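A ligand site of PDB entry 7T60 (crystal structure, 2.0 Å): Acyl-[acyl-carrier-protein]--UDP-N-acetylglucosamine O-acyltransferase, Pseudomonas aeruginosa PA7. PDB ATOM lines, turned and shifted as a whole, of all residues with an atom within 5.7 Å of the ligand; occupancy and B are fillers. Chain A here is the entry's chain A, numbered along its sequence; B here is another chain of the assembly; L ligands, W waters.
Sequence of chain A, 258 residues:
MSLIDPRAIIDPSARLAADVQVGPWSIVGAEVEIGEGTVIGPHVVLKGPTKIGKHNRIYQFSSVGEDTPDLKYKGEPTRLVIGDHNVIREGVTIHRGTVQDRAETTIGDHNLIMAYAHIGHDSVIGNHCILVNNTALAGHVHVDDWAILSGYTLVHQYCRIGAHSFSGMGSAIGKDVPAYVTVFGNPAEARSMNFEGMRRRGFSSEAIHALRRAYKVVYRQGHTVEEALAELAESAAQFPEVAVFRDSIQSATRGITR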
ATOM      1  N   MET A 114     -20.055 -34.497 -18.402  1.00  0.00           N
ATOM      2  CA  MET A 114     -20.702 -34.914 -17.144  1.00  0.00           C
ATOM      3  C   MET A 114     -21.349 -36.268 -17.368  1.00  0.00           C
ATOM      4  O   MET A 114     -21.316 -36.868 -18.508  1.00  0.00           O
ATOM      5  CB  MET A 114     -21.684 -33.869 -16.629  1.00  0.00           C
ATOM      6  CG  MET A 114     -21.023 -32.550 -16.313  1.00  0.00           C
ATOM      7  SD  MET A 114     -22.196 -31.395 -15.530  1.00  0.00           S
ATOM      8  CE  MET A 114     -21.283 -29.856 -15.540  1.00  0.00           C
ATOM      9  N   ILE A 130     -18.898 -27.533 -21.976  1.00  0.00           N
ATOM     10  CA  ILE A 130     -19.546 -28.332 -20.891  1.00  0.00           C
ATOM     11  C   ILE A 130     -20.706 -29.106 -21.525  1.00  0.00           C
ATOM     12  O   ILE A 130     -21.598 -28.464 -22.125  1.00  0.00           O
ATOM     13  CB  ILE A 130     -20.034 -27.435 -19.728  1.00  0.00           C
ATOM     14  CG1 ILE A 130     -18.937 -26.548 -19.135  1.00  0.00           C
ATOM     15  CG2 ILE A 130     -20.699 -28.294 -18.656  1.00  0.00           C
ATOM     16  CD1 ILE A 130     -19.439 -25.546 -18.128  1.00  0.00           C
ATOM     17  N   VAL A 132     -23.466 -31.424 -20.160  1.00  0.00           N
ATOM     18  CA  VAL A 132     -24.157 -31.736 -18.877  1.00  0.00           C
ATOM     19  C   VAL A 132     -24.650 -33.198 -18.938  1.00  0.00           C
ATOM     20  O   VAL A 132     -24.718 -33.743 -20.013  1.00  0.00           O
ATOM     21  CB  VAL A 132     -25.202 -30.634 -18.601  1.00  0.00           C
ATOM     22  CG1 VAL A 132     -26.035 -30.765 -17.341  1.00  0.00           C
ATOM     23  CG2 VAL A 132     -24.532 -29.272 -18.590  1.00  0.00           C
ATOM     24  N   ASN A 133     -25.060 -33.772 -17.817  1.00  0.00           N
ATOM     25  CA  ASN A 133     -25.439 -35.199 -17.705  1.00  0.00           C
ATOM     26  C   ASN A 133     -26.407 -35.630 -18.801  1.00  0.00           C
ATOM     27  O   ASN A 133     -27.361 -34.909 -19.082  1.00  0.00           O
ATOM     28  CB  ASN A 133     -26.234 -35.436 -16.419  1.00  0.00           C
ATOM     29  CG  ASN A 133     -25.509 -35.090 -15.130  1.00  0.00           C
ATOM     30  OD1 ASN A 133     -24.800 -34.111 -15.061  1.00  0.00           O
ATOM     31  ND2 ASN A 133     -25.733 -35.881 -14.105  1.00  0.00           N
ATOM     32  N   ILE A 148     -22.134 -24.742 -24.115  1.00  0.00           N
ATOM     33  CA  ILE A 148     -22.771 -25.483 -22.997  1.00  0.00           C
ATOM     34  C   ILE A 148     -23.986 -26.207 -23.545  1.00  0.00           C
ATOM     35  O   ILE A 148     -24.905 -25.556 -24.057  1.00  0.00           O
ATOM     36  CB  ILE A 148     -23.126 -24.557 -21.835  1.00  0.00           C
ATOM     37  CG1 ILE A 148     -21.867 -23.876 -21.292  1.00  0.00           C
ATOM     38  CG2 ILE A 148     -23.898 -25.332 -20.770  1.00  0.00           C
ATOM     39  CD1 ILE A 148     -22.095 -22.947 -20.105  1.00  0.00           C
ATOM     40  N   SER A 150     -26.957 -28.289 -22.055  1.00  0.00           N
ATOM     41  CA  SER A 150     -27.533 -28.655 -20.739  1.00  0.00           C
ATOM     42  C   SER A 150     -28.021 -30.122 -20.705  1.00  0.00           C
ATOM     43  O   SER A 150     -27.926 -30.855 -21.700  1.00  0.00           O
ATOM     44  CB  SER A 150     -28.565 -27.657 -20.244  1.00  0.00           C
ATOM     45  OG  SER A 150     -28.740 -27.869 -18.857  1.00  0.00           O
ATOM     46  N   GLY A 151     -28.475 -30.567 -19.534  1.00  0.00           N
ATOM     47  CA  GLY A 151     -28.761 -31.986 -19.281  1.00  0.00           C
ATOM     48  C   GLY A 151     -29.687 -32.556 -20.334  1.00  0.00           C
ATOM     49  O   GLY A 151     -30.754 -31.962 -20.654  1.00  0.00           O
ATOM     50  N   TYR A 152     -29.385 -33.746 -20.806  1.00  0.00           N
ATOM     51  CA  TYR A 152     -30.337 -34.495 -21.631  1.00  0.00           C
ATOM     52  C   TYR A 152     -30.536 -33.773 -22.961  1.00  0.00           C
ATOM     53  O   TYR A 152     -31.620 -33.937 -23.536  1.00  0.00           O
ATOM     54  CB  TYR A 152     -31.609 -34.749 -20.835  1.00  0.00           C
ATOM     55  CG  TYR A 152     -31.412 -35.722 -19.711  1.00  0.00           C
ATOM     56  CD1 TYR A 152     -30.801 -35.360 -18.525  1.00  0.00           C
ATOM     57  CD2 TYR A 152     -31.817 -37.031 -19.883  1.00  0.00           C
ATOM     58  CE1 TYR A 152     -30.573 -36.293 -17.522  1.00  0.00           C
ATOM     59  CE2 TYR A 152     -31.611 -37.966 -18.887  1.00  0.00           C
ATOM     60  CZ  TYR A 152     -31.005 -37.596 -17.700  1.00  0.00           C
ATOM     61  OH  TYR A 152     -30.809 -38.541 -16.761  1.00  0.00           O
ATOM     62  N   PHE A 166     -25.673 -22.036 -25.942  1.00  0.00           N
ATOM     63  CA  PHE A 166     -26.312 -22.692 -24.770  1.00  0.00           C
ATOM     64  C   PHE A 166     -27.579 -23.388 -25.233  1.00  0.00           C
ATOM     65  O   PHE A 166     -28.450 -22.732 -25.846  1.00  0.00           O
ATOM     66  CB  PHE A 166     -26.600 -21.710 -23.654  1.00  0.00           C
ATOM     67  CG  PHE A 166     -27.266 -22.298 -22.437  1.00  0.00           C
ATOM     68  CD1 PHE A 166     -26.529 -22.824 -21.402  1.00  0.00           C
ATOM     69  CD2 PHE A 166     -28.646 -22.350 -22.364  1.00  0.00           C
ATOM     70  CE1 PHE A 166     -27.153 -23.388 -20.306  1.00  0.00           C
ATOM     71  CE2 PHE A 166     -29.266 -22.948 -21.283  1.00  0.00           C
ATOM     72  CZ  PHE A 166     -28.531 -23.438 -20.242  1.00  0.00           C
ATOM     73  N   SER A 167     -27.652 -24.697 -24.968  1.00  0.00           N
ATOM     74  CA  SER A 167     -28.883 -25.514 -25.135  1.00  0.00           C
ATOM     75  C   SER A 167     -29.524 -25.778 -23.769  1.00  0.00           C
ATOM     76  O   SER A 167     -28.826 -26.189 -22.842  1.00  0.00           O
ATOM     77  CB  SER A 167     -28.553 -26.790 -25.791  1.00  0.00           C
ATOM     78  OG  SER A 167     -28.073 -27.673 -24.806  1.00  0.00           O
ATOM     79  N   GLY A 168     -30.823 -25.554 -23.642  1.00  0.00           N
ATOM     80  CA  GLY A 168     -31.589 -25.823 -22.406  1.00  0.00           C
ATOM     81  C   GLY A 168     -31.812 -27.308 -22.197  1.00  0.00           C
ATOM     82  O   GLY A 168     -31.703 -28.117 -23.190  1.00  0.00           O
ATOM     83  N   MET A 169     -32.063 -27.662 -20.957  1.00  0.00           N
ATOM     84  CA  MET A 169     -32.207 -29.075 -20.548  1.00  0.00           C
ATOM     85  C   MET A 169     -33.291 -29.733 -21.396  1.00  0.00           C
ATOM     86  O   MET A 169     -34.379 -29.138 -21.627  1.00  0.00           O
ATOM     87  CB  MET A 169     -32.489 -29.211 -19.053  1.00  0.00           C
ATOM     88  CG  MET A 169     -33.703 -28.468 -18.553  1.00  0.00           C
ATOM     89  SD  MET A 169     -33.932 -28.812 -16.781  1.00  0.00           S
ATOM     90  CE  MET A 169     -35.528 -28.001 -16.575  1.00  0.00           C
ATOM     91  N   PHE A 184     -33.928 -23.866 -26.969  1.00  0.00           N
ATOM     92  CA  PHE A 184     -34.814 -24.590 -26.033  1.00  0.00           C
ATOM     93  C   PHE A 184     -35.825 -25.414 -26.833  1.00  0.00           C
ATOM     94  O   PHE A 184     -36.232 -24.969 -27.916  1.00  0.00           O
ATOM     95  CB  PHE A 184     -35.513 -23.626 -25.075  1.00  0.00           C
ATOM     96  CG  PHE A 184     -34.563 -22.806 -24.239  1.00  0.00           C
ATOM     97  CD1 PHE A 184     -34.023 -21.636 -24.743  1.00  0.00           C
ATOM     98  CD2 PHE A 184     -34.167 -23.240 -22.980  1.00  0.00           C
ATOM     99  CE1 PHE A 184     -33.124 -20.878 -23.995  1.00  0.00           C
ATOM    100  CE2 PHE A 184     -33.268 -22.482 -22.231  1.00  0.00           C
ATOM    101  CZ  PHE A 184     -32.771 -21.293 -22.723  1.00  0.00           C
ATOM    102  N   HIS B 118     -30.009 -39.203 -10.771  1.00  0.00           N
ATOM    103  CA  HIS B 118     -28.904 -38.306 -10.385  1.00  0.00           C
ATOM    104  C   HIS B 118     -29.425 -37.375  -9.299  1.00  0.00           C
ATOM    105  O   HIS B 118     -30.437 -36.691  -9.527  1.00  0.00           O
ATOM    106  CB  HIS B 118     -28.369 -37.479 -11.560  1.00  0.00           C
ATOM    107  CG  HIS B 118     -27.401 -36.454 -11.077  1.00  0.00           C
ATOM    108  ND1 HIS B 118     -26.178 -36.814 -10.553  1.00  0.00           N
ATOM    109  CD2 HIS B 118     -27.490 -35.109 -11.015  1.00  0.00           C
ATOM    110  CE1 HIS B 118     -25.540 -35.715 -10.212  1.00  0.00           C
ATOM    111  NE2 HIS B 118     -26.333 -34.643 -10.480  1.00  0.00           N
ATOM    112  N   ALA B 136     -33.117 -36.502 -12.783  1.00  0.00           N
ATOM    113  CA  ALA B 136     -31.907 -35.707 -12.520  1.00  0.00           C
ATOM    114  C   ALA B 136     -32.263 -34.433 -11.725  1.00  0.00           C
ATOM    115  O   ALA B 136     -33.156 -33.665 -12.181  1.00  0.00           O
ATOM    116  CB  ALA B 136     -31.241 -35.388 -13.819  1.00  0.00           C
ATOM    117  N   LEU B 137     -31.702 -34.322 -10.516  1.00  0.00           N
ATOM    118  CA  LEU B 137     -31.824 -33.103  -9.665  1.00  0.00           C
ATOM    119  C   LEU B 137     -30.507 -32.374  -9.832  1.00  0.00           C
ATOM    120  O   LEU B 137     -29.465 -32.931  -9.378  1.00  0.00           O
ATOM    121  CB  LEU B 137     -32.071 -33.471  -8.206  1.00  0.00           C
ATOM    122  CG  LEU B 137     -33.076 -34.589  -7.916  1.00  0.00           C
ATOM    123  CD1 LEU B 137     -33.332 -34.672  -6.417  1.00  0.00           C
ATOM    124  CD2 LEU B 137     -34.390 -34.396  -8.668  1.00  0.00           C
ATOM    125  N   ALA B 138     -30.537 -31.182 -10.417  1.00  0.00           N
ATOM    126  CA  ALA B 138     -29.346 -30.399 -10.757  1.00  0.00           C
ATOM    127  C   ALA B 138     -28.557 -30.046  -9.481  1.00  0.00           C
ATOM    128  O   ALA B 138     -27.333 -30.028  -9.550  1.00  0.00           O
ATOM    129  CB  ALA B 138     -29.687 -29.173 -11.558  1.00  0.00           C
ATOM    130  N   LEU B 154     -36.348 -33.886 -15.188  1.00  0.00           N
ATOM    131  CA  LEU B 154     -35.200 -32.993 -15.042  1.00  0.00           C
ATOM    132  C   LEU B 154     -35.602 -31.865 -14.093  1.00  0.00           C
ATOM    133  O   LEU B 154     -36.713 -31.321 -14.307  1.00  0.00           O
ATOM    134  CB  LEU B 154     -34.806 -32.426 -16.411  1.00  0.00           C
ATOM    135  CG  LEU B 154     -34.666 -33.460 -17.512  1.00  0.00           C
ATOM    136  CD1 LEU B 154     -34.231 -32.777 -18.799  1.00  0.00           C
ATOM    137  CD2 LEU B 154     -33.708 -34.572 -17.101  1.00  0.00           C
ATOM    138  N   VAL B 155     -34.795 -31.582 -13.074  1.00  0.00           N
ATOM    139  CA  VAL B 155     -35.132 -30.505 -12.104  1.00  0.00           C
ATOM    140  C   VAL B 155     -33.979 -29.514 -12.016  1.00  0.00           C
ATOM    141  O   VAL B 155     -32.819 -29.921 -11.610  1.00  0.00           O
ATOM    142  CB  VAL B 155     -35.513 -31.050 -10.708  1.00  0.00           C
ATOM    143  CG1 VAL B 155     -35.992 -29.928  -9.813  1.00  0.00           C
ATOM    144  CG2 VAL B 155     -36.539 -32.150 -10.831  1.00  0.00           C
ATOM    145  N   HIS B 156     -34.305 -28.260 -12.337  1.00  0.00           N
ATOM    146  CA  HIS B 156     -33.401 -27.086 -12.195  1.00  0.00           C
ATOM    147  C   HIS B 156     -32.929 -26.942 -10.744  1.00  0.00           C
ATOM    148  O   HIS B 156     -33.661 -27.306  -9.795  1.00  0.00           O
ATOM    149  CB  HIS B 156     -34.088 -25.832 -12.772  1.00  0.00           C
ATOM    150  CG  HIS B 156     -33.239 -24.634 -12.967  1.00  0.00           C
ATOM    151  ND1 HIS B 156     -32.861 -23.807 -11.911  1.00  0.00           N
ATOM    152  CD2 HIS B 156     -32.735 -24.068 -14.085  1.00  0.00           C
ATOM    153  CE1 HIS B 156     -32.112 -22.809 -12.383  1.00  0.00           C
ATOM    154  NE2 HIS B 156     -32.047 -22.934 -13.704  1.00  0.00           N
ATOM    155  N   GLN B 157     -31.750 -26.365 -10.574  1.00  0.00           N
ATOM    156  CA  GLN B 157     -31.195 -26.144  -9.214  1.00  0.00           C
ATOM    157  C   GLN B 157     -32.131 -25.215  -8.442  1.00  0.00           C
ATOM    158  O   GLN B 157     -32.704 -24.368  -9.049  1.00  0.00           O
ATOM    159  CB  GLN B 157     -29.840 -25.459  -9.336  1.00  0.00           C
ATOM    160  CG  GLN B 157     -28.652 -26.407  -9.360  1.00  0.00           C
ATOM    161  CD  GLN B 157     -27.340 -25.692  -9.185  1.00  0.00           C
ATOM    162  OE1 GLN B 157     -27.226 -24.740  -8.435  1.00  0.00           O
ATOM    163  NE2 GLN B 157     -26.318 -26.137  -9.893  1.00  0.00           N
ATOM    164  N   TYR B 158     -32.302 -25.476  -7.145  1.00  0.00           N
ATOM    165  CA  TYR B 158     -33.008 -24.613  -6.151  1.00  0.00           C
ATOM    166  C   TYR B 158     -34.526 -24.823  -6.202  1.00  0.00           C
ATOM    167  O   TYR B 158     -35.253 -24.234  -5.392  1.00  0.00           O
ATOM    168  CB  TYR B 158     -32.706 -23.122  -6.348  1.00  0.00           C
ATOM    169  CG  TYR B 158     -31.270 -22.778  -6.058  1.00  0.00           C
ATOM    170  CD1 TYR B 158     -30.776 -22.842  -4.758  1.00  0.00           C
ATOM    171  CD2 TYR B 158     -30.393 -22.438  -7.076  1.00  0.00           C
ATOM    172  CE1 TYR B 158     -29.440 -22.566  -4.485  1.00  0.00           C
ATOM    173  CE2 TYR B 158     -29.054 -22.173  -6.824  1.00  0.00           C
ATOM    174  CZ  TYR B 158     -28.582 -22.227  -5.518  1.00  0.00           C
ATOM    175  OH  TYR B 158     -27.267 -21.930  -5.258  1.00  0.00           O
HETATM  176  O1  LIG L   1     -24.744 -29.065 -14.645  1.00  0.00           O
HETATM  177  C1  LIG L   1     -25.851 -28.825 -14.348  1.00  0.00           C
HETATM  178  C2  LIG L   1     -26.690 -29.998 -13.990  1.00  0.00           C
HETATM  179  C3  LIG L   1     -26.279 -31.160 -13.391  1.00  0.00           C
HETATM  180  C4  LIG L   1     -27.121 -32.262 -13.358  1.00  0.00           C
HETATM  181  C5  LIG L   1     -28.315 -32.310 -14.019  1.00  0.00           C
HETATM  182  C6  LIG L   1     -28.722 -31.196 -14.677  1.00  0.00           C
HETATM  183  C7  LIG L   1     -30.079 -31.248 -15.372  1.00  0.00           C
HETATM  184  F1  LIG L   1     -31.064 -30.952 -14.457  1.00  0.00           F
HETATM  185  F2  LIG L   1     -30.241 -32.535 -15.820  1.00  0.00           F
HETATM  186  F3  LIG L   1     -30.163 -30.377 -16.439  1.00  0.00           F
HETATM  187  C8  LIG L   1     -27.894 -30.080 -14.732  1.00  0.00           C
HETATM  188  N1  LIG L   1     -26.338 -27.535 -14.646  1.00  0.00           N
HETATM  189  C9  LIG L   1     -25.688 -26.457 -15.405  1.00  0.00           C
HETATM  190  C10 LIG L   1     -26.600 -25.452 -15.642  1.00  0.00           C
HETATM  191  C11 LIG L   1     -26.278 -24.331 -16.423  1.00  0.00           C
HETATM  192  C12 LIG L   1     -25.074 -24.350 -17.111  1.00  0.00           C
HETATM  193  C13 LIG L   1     -24.224 -25.414 -17.005  1.00  0.00           C
HETATM  194  C14 LIG L   1     -24.530 -26.486 -16.191  1.00  0.00           C
HETATM  195  C15 LIG L   1     -27.698 -25.727 -14.697  1.00  0.00           C
HETATM  196  C16 LIG L   1     -28.830 -25.964 -15.715  1.00  0.00           C
HETATM  197  N2  LIG L   1     -29.430 -24.746 -16.221  1.00  0.00           N
HETATM  198  C17 LIG L   1     -30.387 -24.840 -17.222  1.00  0.00           C
HETATM  199  N3  LIG L   1     -30.445 -25.876 -18.033  1.00  0.00           N
HETATM  200  N4  LIG L   1     -31.485 -25.647 -18.903  1.00  0.00           N
HETATM  201  N5  LIG L   1     -32.015 -24.459 -18.598  1.00  0.00           N
HETATM  202  N6  LIG L   1     -31.312 -23.944 -17.562  1.00  0.00           N
HETATM  203  O2  LIG L   1     -29.235 -27.096 -16.006  1.00  0.00           O
HETATM  204  N7  LIG L   1     -28.070 -24.642 -13.850  1.00  0.00           N
HETATM  205  C18 LIG L   1     -27.310 -23.486 -13.531  1.00  0.00           C
HETATM  206  C19 LIG L   1     -27.987 -22.778 -12.364  1.00  0.00           C
HETATM  207  C20 LIG L   1     -27.166 -22.609 -11.075  1.00  0.00           C
HETATM  208  C21 LIG L   1     -28.471 -21.343 -12.733  1.00  0.00           C
HETATM  209  O3  LIG L   1     -29.078 -23.626 -12.005  1.00  0.00           O
HETATM  210  C22 LIG L   1     -29.199 -24.686 -12.942  1.00  0.00           C
HETATM  211  O4  LIG L   1     -30.002 -25.520 -12.931  1.00  0.00           O
HETATM  212  C23 LIG L   1     -27.660 -27.163 -14.325  1.00  0.00           C
HETATM  213  O   HOH W   1     -26.003 -28.398 -11.434  1.00  0.00           O
HETATM  214  O   HOH W   2     -25.565 -32.164 -10.180  1.00  0.00           O
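SD of Met 114 lies close to OD1 of Asn 133. N of Ser 167 sits at hydrogen-bond distance from O of Ile 148, 3.0 Å away. N of Val 155 of chain B is in hydrogen-bond range of O of Ala 136 of chain B, at 2.8 Å. N of Leu 137 of chain B is in hydrogen-bond range of O of His 118 of chain B, 2.9 Å away. The backbone NH of Ala 138 of chain B lies within hydrogen-bond range of the backbone carbonyl oxygen of Val 155 of chain B (2.9 Å). The backbone NH (N) of Tyr 152 sits at hydrogen-bond distance from the backbone carbonyl oxygen (O) of Asn 133. N of Ser 150 is in hydrogen-bond range of O of Ser 167.
NE2 of His 156 of chain B lies close to O4 of the ligand. The backbone NH (N) of Met 169 lies within hydrogen-bond range of a nitrogen (N4) of the ligand, at 2.9 Å. The backbone NH of Gln 157 of chain B is in hydrogen-bond range of an oxygen (O4) of the ligand (3.1 Å). N3 of the ligand lies within hydrogen-bond range of OG of Ser 150 (2.7 Å).
The side-chain sulfur of Met 114 lies close to an oxygen (O1) of the ligand (3.6 Å). The backbone carbonyl oxygen (O) of Val 155 of chain B sits close to a fluorine (F1) of the ligand (3.5 Å). Residues that only touch the ligand: Val 132, Asn 133, Ile 148, Gly 151, Tyr 152, Phe 166, Gly 168, His 118 of chain B, Ala 136 of chain B and Ala 138 of chain B. Hydrophobic or aromatic side chains that line the ligand: Met 114, Val 132, Ile 148, Tyr 152, Phe 166, Met 169, His 118 of chain B, Ala 136 of chain B, Ala 138 of chain B and His 156 of chain B. Of the 22 residues printed, 16 come within 4 Å of the ligand.
Water W1 bridges NE2 of Gln 157 of chain B (2.8 Å) and O of Ala 138 of chain B (2.8 Å). Water W2 bridges NE2 of His 118 of chain B (2.6 Å) and O of Ala 138 of chain B (2.8 Å).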
